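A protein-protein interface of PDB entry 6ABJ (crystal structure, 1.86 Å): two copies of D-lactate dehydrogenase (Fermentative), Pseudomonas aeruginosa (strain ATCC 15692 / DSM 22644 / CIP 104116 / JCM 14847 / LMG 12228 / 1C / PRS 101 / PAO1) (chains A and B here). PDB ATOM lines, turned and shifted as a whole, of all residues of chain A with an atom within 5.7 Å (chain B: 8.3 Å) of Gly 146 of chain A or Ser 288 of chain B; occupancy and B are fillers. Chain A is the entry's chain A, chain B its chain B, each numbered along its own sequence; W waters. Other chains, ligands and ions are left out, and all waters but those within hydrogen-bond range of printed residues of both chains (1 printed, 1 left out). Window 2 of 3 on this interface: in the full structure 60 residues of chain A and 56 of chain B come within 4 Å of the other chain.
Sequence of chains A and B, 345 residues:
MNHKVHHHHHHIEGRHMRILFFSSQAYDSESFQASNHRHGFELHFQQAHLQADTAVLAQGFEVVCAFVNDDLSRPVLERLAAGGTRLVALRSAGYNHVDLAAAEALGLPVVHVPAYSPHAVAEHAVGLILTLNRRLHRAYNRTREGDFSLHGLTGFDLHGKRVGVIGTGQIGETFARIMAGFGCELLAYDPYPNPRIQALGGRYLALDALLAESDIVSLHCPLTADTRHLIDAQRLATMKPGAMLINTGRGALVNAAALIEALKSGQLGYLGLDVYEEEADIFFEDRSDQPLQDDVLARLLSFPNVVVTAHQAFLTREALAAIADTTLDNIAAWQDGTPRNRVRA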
ATOM      1  N   ARG A 142     -19.701  28.327  27.084  1.00  0.00           N
ATOM      2  CA  ARG A 142     -18.392  27.648  27.050  1.00  0.00           C
ATOM      3  C   ARG A 142     -17.620  27.725  28.354  1.00  0.00           C
ATOM      4  O   ARG A 142     -17.183  26.713  28.891  1.00  0.00           O
ATOM      5  CB  ARG A 142     -17.535  28.221  25.913  1.00  0.00           C
ATOM      6  CG  ARG A 142     -18.039  27.891  24.536  1.00  0.00           C
ATOM      7  CD  ARG A 142     -16.977  28.358  23.527  1.00  0.00           C
ATOM      8  NE  ARG A 142     -17.541  28.324  22.166  1.00  0.00           N
ATOM      9  CZ  ARG A 142     -16.898  28.675  21.058  1.00  0.00           C
ATOM     10  NH1 ARG A 142     -15.638  29.147  21.115  1.00  0.00           N
ATOM     11  NH2 ARG A 142     -17.524  28.541  19.871  1.00  0.00           N
ATOM     12  N   THR A 143     -17.370  28.924  28.823  1.00  0.00           N
ATOM     13  CA  THR A 143     -16.539  29.074  29.964  1.00  0.00           C
ATOM     14  C   THR A 143     -17.075  28.451  31.219  1.00  0.00           C
ATOM     15  O   THR A 143     -16.315  27.906  32.006  1.00  0.00           O
ATOM     16  CB  THR A 143     -16.089  30.555  30.232  1.00  0.00           C
ATOM     17  OG1 THR A 143     -17.186  31.368  30.565  1.00  0.00           O
ATOM     18  CG2 THR A 143     -15.363  31.162  29.043  1.00  0.00           C
ATOM     19  N   ARG A 144     -18.384  28.490  31.376  1.00  0.00           N
ATOM     20  CA  ARG A 144     -19.011  27.872  32.513  1.00  0.00           C
ATOM     21  C   ARG A 144     -18.683  26.377  32.583  1.00  0.00           C
ATOM     22  O   ARG A 144     -18.632  25.801  33.671  1.00  0.00           O
ATOM     23  CB  ARG A 144     -20.519  28.004  32.374  1.00  0.00           C
ATOM     24  CG  ARG A 144     -21.185  28.820  33.465  1.00  0.00           C
ATOM     25  CD  ARG A 144     -22.660  28.471  33.576  1.00  0.00           C
ATOM     26  NE  ARG A 144     -23.248  28.071  32.297  1.00  0.00           N
ATOM     27  CZ  ARG A 144     -24.403  27.439  32.170  1.00  0.00           C
ATOM     28  NH1 ARG A 144     -25.114  27.131  33.245  1.00  0.00           N
ATOM     29  NH2 ARG A 144     -24.854  27.114  30.964  1.00  0.00           N
ATOM     30  N   GLU A 145     -18.481  25.751  31.422  1.00  0.00           N
ATOM     31  CA  GLU A 145     -18.151  24.351  31.383  1.00  0.00           C
ATOM     32  C   GLU A 145     -16.626  24.075  31.191  1.00  0.00           C
ATOM     33  O   GLU A 145     -16.191  22.937  31.022  1.00  0.00           O
ATOM     34  CB  GLU A 145     -19.030  23.607  30.332  1.00  0.00           C
ATOM     35  CG  GLU A 145     -18.774  23.965  28.861  1.00  0.00           C
ATOM     36  CD  GLU A 145     -19.639  23.228  27.860  1.00  0.00           C
ATOM     37  OE1 GLU A 145     -20.102  22.126  28.187  1.00  0.00           O
ATOM     38  OE2 GLU A 145     -19.880  23.771  26.736  1.00  0.00           O
ATOM     39  N   GLY A 146     -15.816  25.109  31.318  1.00  0.00           N
ATOM     40  CA  GLY A 146     -14.342  24.937  31.161  1.00  0.00           C
ATOM     41  C   GLY A 146     -13.860  24.906  29.744  1.00  0.00           C
ATOM     42  O   GLY A 146     -12.756  24.437  29.495  1.00  0.00           O
ATOM     43  N   ASP A 147     -14.689  25.348  28.797  1.00  0.00           N
ATOM     44  CA  ASP A 147     -14.246  25.529  27.437  1.00  0.00           C
ATOM     45  C   ASP A 147     -13.821  26.982  27.265  1.00  0.00           C
ATOM     46  O   ASP A 147     -14.673  27.923  27.180  1.00  0.00           O
ATOM     47  CB  ASP A 147     -15.337  25.191  26.463  1.00  0.00           C
ATOM     48  CG  ASP A 147     -14.927  25.390  25.017  1.00  0.00           C
ATOM     49  OD1 ASP A 147     -13.740  25.719  24.773  1.00  0.00           O
ATOM     50  OD2 ASP A 147     -15.804  25.182  24.123  1.00  0.00           O
ATOM     51  N   PHE A 148     -12.494  27.179  27.246  1.00  0.00           N
ATOM     52  CA  PHE A 148     -11.920  28.518  27.127  1.00  0.00           C
ATOM     53  C   PHE A 148     -11.396  28.781  25.716  1.00  0.00           C
ATOM     54  O   PHE A 148     -10.587  29.667  25.505  1.00  0.00           O
ATOM     55  CB  PHE A 148     -10.795  28.666  28.150  1.00  0.00           C
ATOM     56  CG  PHE A 148     -11.219  28.356  29.555  1.00  0.00           C
ATOM     57  CD1 PHE A 148     -12.026  29.238  30.261  1.00  0.00           C
ATOM     58  CD2 PHE A 148     -10.832  27.190  30.165  1.00  0.00           C
ATOM     59  CE1 PHE A 148     -12.461  28.964  31.516  1.00  0.00           C
ATOM     60  CE2 PHE A 148     -11.253  26.909  31.452  1.00  0.00           C
ATOM     61  CZ  PHE A 148     -12.092  27.775  32.120  1.00  0.00           C
ATOM     62  N   ILE B 282      -4.637  28.200  31.392  1.00  0.00           N
ATOM     63  CA  ILE B 282      -6.059  27.793  31.496  1.00  0.00           C
ATOM     64  C   ILE B 282      -6.797  28.153  30.218  1.00  0.00           C
ATOM     65  O   ILE B 282      -7.454  27.332  29.633  1.00  0.00           O
ATOM     66  CB  ILE B 282      -6.798  28.530  32.645  1.00  0.00           C
ATOM     67  CG1 ILE B 282      -6.077  28.386  33.992  1.00  0.00           C
ATOM     68  CG2 ILE B 282      -8.257  28.038  32.755  1.00  0.00           C
ATOM     69  CD1 ILE B 282      -6.192  27.033  34.640  1.00  0.00           C
ATOM     70  N   PHE B 283      -6.701  29.418  29.849  1.00  0.00           N
ATOM     71  CA  PHE B 283      -7.397  29.948  28.740  1.00  0.00           C
ATOM     72  C   PHE B 283      -6.885  29.465  27.383  1.00  0.00           C
ATOM     73  O   PHE B 283      -5.861  28.827  27.265  1.00  0.00           O
ATOM     74  CB  PHE B 283      -7.338  31.454  28.791  1.00  0.00           C
ATOM     75  CG  PHE B 283      -8.201  32.128  29.875  1.00  0.00           C
ATOM     76  CD1 PHE B 283      -8.985  31.435  30.784  1.00  0.00           C
ATOM     77  CD2 PHE B 283      -8.265  33.522  29.889  1.00  0.00           C
ATOM     78  CE1 PHE B 283      -9.756  32.150  31.719  1.00  0.00           C
ATOM     79  CE2 PHE B 283      -8.993  34.215  30.814  1.00  0.00           C
ATOM     80  CZ  PHE B 283      -9.783  33.533  31.697  1.00  0.00           C
ATOM     81  N   PHE B 284      -7.683  29.761  26.370  1.00  0.00           N
ATOM     82  CA  PHE B 284      -7.402  29.495  24.981  1.00  0.00           C
ATOM     83  C   PHE B 284      -7.403  28.048  24.631  1.00  0.00           C
ATOM     84  O   PHE B 284      -6.843  27.677  23.623  1.00  0.00           O
ATOM     85  CB  PHE B 284      -6.034  30.107  24.589  1.00  0.00           C
ATOM     86  CG  PHE B 284      -5.825  31.484  25.125  1.00  0.00           C
ATOM     87  CD1 PHE B 284      -6.606  32.516  24.657  1.00  0.00           C
ATOM     88  CD2 PHE B 284      -4.902  31.725  26.132  1.00  0.00           C
ATOM     89  CE1 PHE B 284      -6.453  33.775  25.168  1.00  0.00           C
ATOM     90  CE2 PHE B 284      -4.740  32.978  26.655  1.00  0.00           C
ATOM     91  CZ  PHE B 284      -5.502  34.011  26.158  1.00  0.00           C
ATOM     92  N   GLU B 285      -7.998  27.223  25.459  1.00  0.00           N
ATOM     93  CA  GLU B 285      -8.066  25.805  25.229  1.00  0.00           C
ATOM     94  C   GLU B 285      -9.432  25.304  25.693  1.00  0.00           C
ATOM     95  O   GLU B 285      -9.935  25.819  26.656  1.00  0.00           O
ATOM     96  CB  GLU B 285      -7.061  25.205  26.166  1.00  0.00           C
ATOM     97  CG  GLU B 285      -6.832  23.713  25.981  1.00  0.00           C
ATOM     98  CD  GLU B 285      -5.538  23.410  25.249  1.00  0.00           C
ATOM     99  OE1 GLU B 285      -5.018  24.320  24.557  1.00  0.00           O
ATOM    100  OE2 GLU B 285      -5.041  22.267  25.406  1.00  0.00           O
ATOM    101  N   ASP B 286      -9.954  24.293  25.058  1.00  0.00           N
ATOM    102  CA  ASP B 286     -11.143  23.628  25.522  1.00  0.00           C
ATOM    103  C   ASP B 286     -10.770  22.612  26.531  1.00  0.00           C
ATOM    104  O   ASP B 286     -10.261  21.559  26.184  1.00  0.00           O
ATOM    105  CB  ASP B 286     -11.875  22.981  24.397  1.00  0.00           C
ATOM    106  CG  ASP B 286     -13.125  22.235  24.840  1.00  0.00           C
ATOM    107  OD1 ASP B 286     -13.470  22.182  26.037  1.00  0.00           O
ATOM    108  OD2 ASP B 286     -13.736  21.647  23.962  1.00  0.00           O
ATOM    109  N   ARG B 287     -10.992  22.955  27.802  1.00  0.00           N
ATOM    110  CA  ARG B 287     -10.725  22.031  28.912  1.00  0.00           C
ATOM    111  C   ARG B 287     -11.980  21.380  29.479  1.00  0.00           C
ATOM    112  O   ARG B 287     -11.989  20.930  30.616  1.00  0.00           O
ATOM    113  CB  ARG B 287      -9.963  22.814  29.977  1.00  0.00           C
ATOM    114  CG  ARG B 287      -8.589  23.264  29.465  1.00  0.00           C
ATOM    115  CD  ARG B 287      -7.814  24.053  30.511  1.00  0.00           C
ATOM    116  NE  ARG B 287      -6.617  24.665  29.919  1.00  0.00           N
ATOM    117  CZ  ARG B 287      -5.502  24.002  29.614  1.00  0.00           C
ATOM    118  NH1 ARG B 287      -5.389  22.710  29.863  1.00  0.00           N
ATOM    119  NH2 ARG B 287      -4.493  24.655  29.059  1.00  0.00           N
ATOM    120  N   SER B 288     -12.999  21.218  28.659  1.00  0.00           N
ATOM    121  CA  SER B 288     -14.321  20.899  29.235  1.00  0.00           C
ATOM    122  C   SER B 288     -14.432  19.402  29.506  1.00  0.00           C
ATOM    123  O   SER B 288     -15.292  18.971  30.189  1.00  0.00           O
ATOM    124  CB  SER B 288     -15.399  21.373  28.280  1.00  0.00           C
ATOM    125  OG  SER B 288     -15.259  20.712  27.055  1.00  0.00           O
ATOM    126  N   ASP B 289     -13.551  18.587  28.884  1.00  0.00           N
ATOM    127  CA  ASP B 289     -13.570  17.160  29.064  1.00  0.00           C
ATOM    128  C   ASP B 289     -12.987  16.692  30.427  1.00  0.00           C
ATOM    129  O   ASP B 289     -13.193  15.542  30.810  1.00  0.00           O
ATOM    130  CB  ASP B 289     -12.849  16.441  27.880  1.00  0.00           C
ATOM    131  CG  ASP B 289     -13.655  16.496  26.545  1.00  0.00           C
ATOM    132  OD1 ASP B 289     -14.904  16.529  26.560  1.00  0.00           O
ATOM    133  OD2 ASP B 289     -13.064  16.392  25.455  1.00  0.00           O
ATOM    134  N   GLN B 290     -12.315  17.577  31.140  1.00  0.00           N
ATOM    135  CA  GLN B 290     -11.622  17.239  32.362  1.00  0.00           C
ATOM    136  C   GLN B 290     -12.010  18.154  33.540  1.00  0.00           C
ATOM    137  O   GLN B 290     -12.289  19.309  33.359  1.00  0.00           O
ATOM    138  CB  GLN B 290     -10.107  17.431  32.120  1.00  0.00           C
ATOM    139  CG  GLN B 290      -9.554  16.659  30.924  1.00  0.00           C
ATOM    140  CD  GLN B 290      -9.668  15.146  31.101  1.00  0.00           C
ATOM    141  OE1 GLN B 290      -9.975  14.414  30.149  1.00  0.00           O
ATOM    142  NE2 GLN B 290      -9.427  14.663  32.320  1.00  0.00           N
ATOM    143  N   PRO B 291     -11.977  17.627  34.764  1.00  0.00           N
ATOM    144  CA  PRO B 291     -12.159  18.495  35.903  1.00  0.00           C
ATOM    145  C   PRO B 291     -11.280  19.649  35.824  1.00  0.00           C
ATOM    146  O   PRO B 291     -10.154  19.559  35.333  1.00  0.00           O
ATOM    147  CB  PRO B 291     -11.775  17.601  37.097  1.00  0.00           C
ATOM    148  CG  PRO B 291     -12.194  16.262  36.669  1.00  0.00           C
ATOM    149  CD  PRO B 291     -11.864  16.210  35.186  1.00  0.00           C
ATOM    150  N   LEU B 292     -11.767  20.779  36.316  1.00  0.00           N
ATOM    151  CA  LEU B 292     -10.977  21.971  36.412  1.00  0.00           C
ATOM    152  C   LEU B 292     -10.232  21.902  37.708  1.00  0.00           C
ATOM    153  O   LEU B 292     -10.847  21.716  38.753  1.00  0.00           O
ATOM    154  CB  LEU B 292     -11.857  23.228  36.459  1.00  0.00           C
ATOM    155  CG  LEU B 292     -11.988  24.251  35.380  1.00  0.00           C
ATOM    156  CD1 LEU B 292     -12.605  25.503  36.026  1.00  0.00           C
ATOM    157  CD2 LEU B 292     -10.683  24.609  34.670  1.00  0.00           C
ATOM    158  N   LEU B 297     -11.232  29.692  40.333  1.00  0.00           N
ATOM    159  CA  LEU B 297     -11.896  29.862  39.069  1.00  0.00           C
ATOM    160  C   LEU B 297     -13.145  29.005  38.977  1.00  0.00           C
ATOM    161  O   LEU B 297     -14.138  29.471  38.478  1.00  0.00           O
ATOM    162  CB  LEU B 297     -10.976  29.498  37.891  1.00  0.00           C
ATOM    163  CG  LEU B 297     -11.529  29.732  36.504  1.00  0.00           C
ATOM    164  CD1 LEU B 297     -11.871  31.188  36.309  1.00  0.00           C
ATOM    165  CD2 LEU B 297     -10.541  29.320  35.424  1.00  0.00           C
ATOM    166  N   LEU B 301     -16.874  30.645  38.242  1.00  0.00           N
ATOM    167  CA  LEU B 301     -17.654  30.248  37.116  1.00  0.00           C
ATOM    168  C   LEU B 301     -19.132  29.824  37.433  1.00  0.00           C
ATOM    169  O   LEU B 301     -19.960  29.979  36.578  1.00  0.00           O
ATOM    170  CB  LEU B 301     -16.996  29.158  36.304  1.00  0.00           C
ATOM    171  CG  LEU B 301     -15.749  29.684  35.565  1.00  0.00           C
ATOM    172  CD1 LEU B 301     -14.880  28.498  35.135  1.00  0.00           C
ATOM    173  CD2 LEU B 301     -16.072  30.574  34.377  1.00  0.00           C
ATOM    174  N   ALA B 310     -12.674  34.402  27.895  1.00  0.00           N
ATOM    175  CA  ALA B 310     -11.342  33.820  27.988  1.00  0.00           C
ATOM    176  C   ALA B 310     -10.311  34.652  27.220  1.00  0.00           C
ATOM    177  O   ALA B 310      -9.805  34.267  26.143  1.00  0.00           O
ATOM    178  CB  ALA B 310     -11.358  32.344  27.595  1.00  0.00           C
HETATM  179  O   HOH W   1     -17.225  20.487  31.214  1.00  0.00           O
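Leu 301 of chain B touches Thr 143 of chain A (CD1 to O, 3.5 Å).
CG of Arg 144 of chain A touches O of Leu 301 of chain B (3.5 Å).
O of Glu 145 of chain A touches CB of Ser 288 of chain B, at 3.3 Å.
Asp 147 of chain A touches Asp 286 of chain B (OD1 to CB, 3.3 Å).
O of Ile 282 of chain B touches CD2 of Phe 148 of chain A (3.4 Å).
CA of Phe 283 of chain B touches CB of Phe 148 of chain A, at 3.7 Å.
Leu 292 of chain B touches Phe 148 of chain A.
Phe 148 of chain A touches Leu 297 of chain B.
Ala 310 of chain B touches Phe 148 of chain A.
Water W1 lies within hydrogen-bond range of the backbone carbonyl oxygen of Ser 288 of chain B and the backbone carbonyl oxygen of Glu 145 of chain A.
No position is printed for both chains.
Of the 13 pairs that touch across the chains among the printed residues, none has its exchanged pair printed and touching as well.
Of the printed residues of chain B, Gly 146 of chain A touches Arg 287 (2.9 Å) and Ser 288 (3.3 Å).
Ser 288 of chain B touches just these residues of chain A: Glu 145 and Gly 146.
Of the printed residues of chain A, Asp 286 of chain B touches Asp 147.
Printed residues of chain B within 4 Å of Arg 144 of chain A: Leu 301 (3.5 Å).
The nearest printed residue of chain B that does not touch Gly 146 of chain A is Asp 286 of chain B (4.01 Å).
N of Asp 147 of chain A is in hydrogen-bond range of O of Arg 142 of chain A.
OG of Ser 288 of chain B lies within hydrogen-bond range of OD1 of Asp 286 of chain B (2.5 Å).
The guanidinium group (NE) of Arg 287 of chain B sits at hydrogen-bond distance from the backbone carbonyl oxygen (O) of Ile 282 of chain B.
The backbone NH (N) of Phe 284 of chain B lies within hydrogen-bond range of the backbone carbonyl oxygen (O) of Phe 148 of chain A, 3.0 Å away.
The backbone carbonyl oxygen (O) of Gly 146 of chain A sits at hydrogen-bond distance from the backbone NH (N) of Arg 287 of chain B (2.9 Å).
The backbone carbonyl oxygen of Gly 146 of chain A is in hydrogen-bond range of the backbone NH of Ser 288 of chain B (3.3 Å).
The backbone carbonyl oxygen of Glu 285 of chain B is in hydrogen-bond range of the backbone NH of Phe 148 of chain A, at 3.0 Å.
Of the 7 printed residues of chain A, 6 touch a printed residue of chain B.
Hydrophobic or aromatic side chains of chain A that line the printed part of chain B: Phe 148.
Hydrophobic or aromatic side chains of chain B that line the printed part of chain A: Ile 282, Phe 283, Leu 292, Leu 297, Leu 301 and Ala 310.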
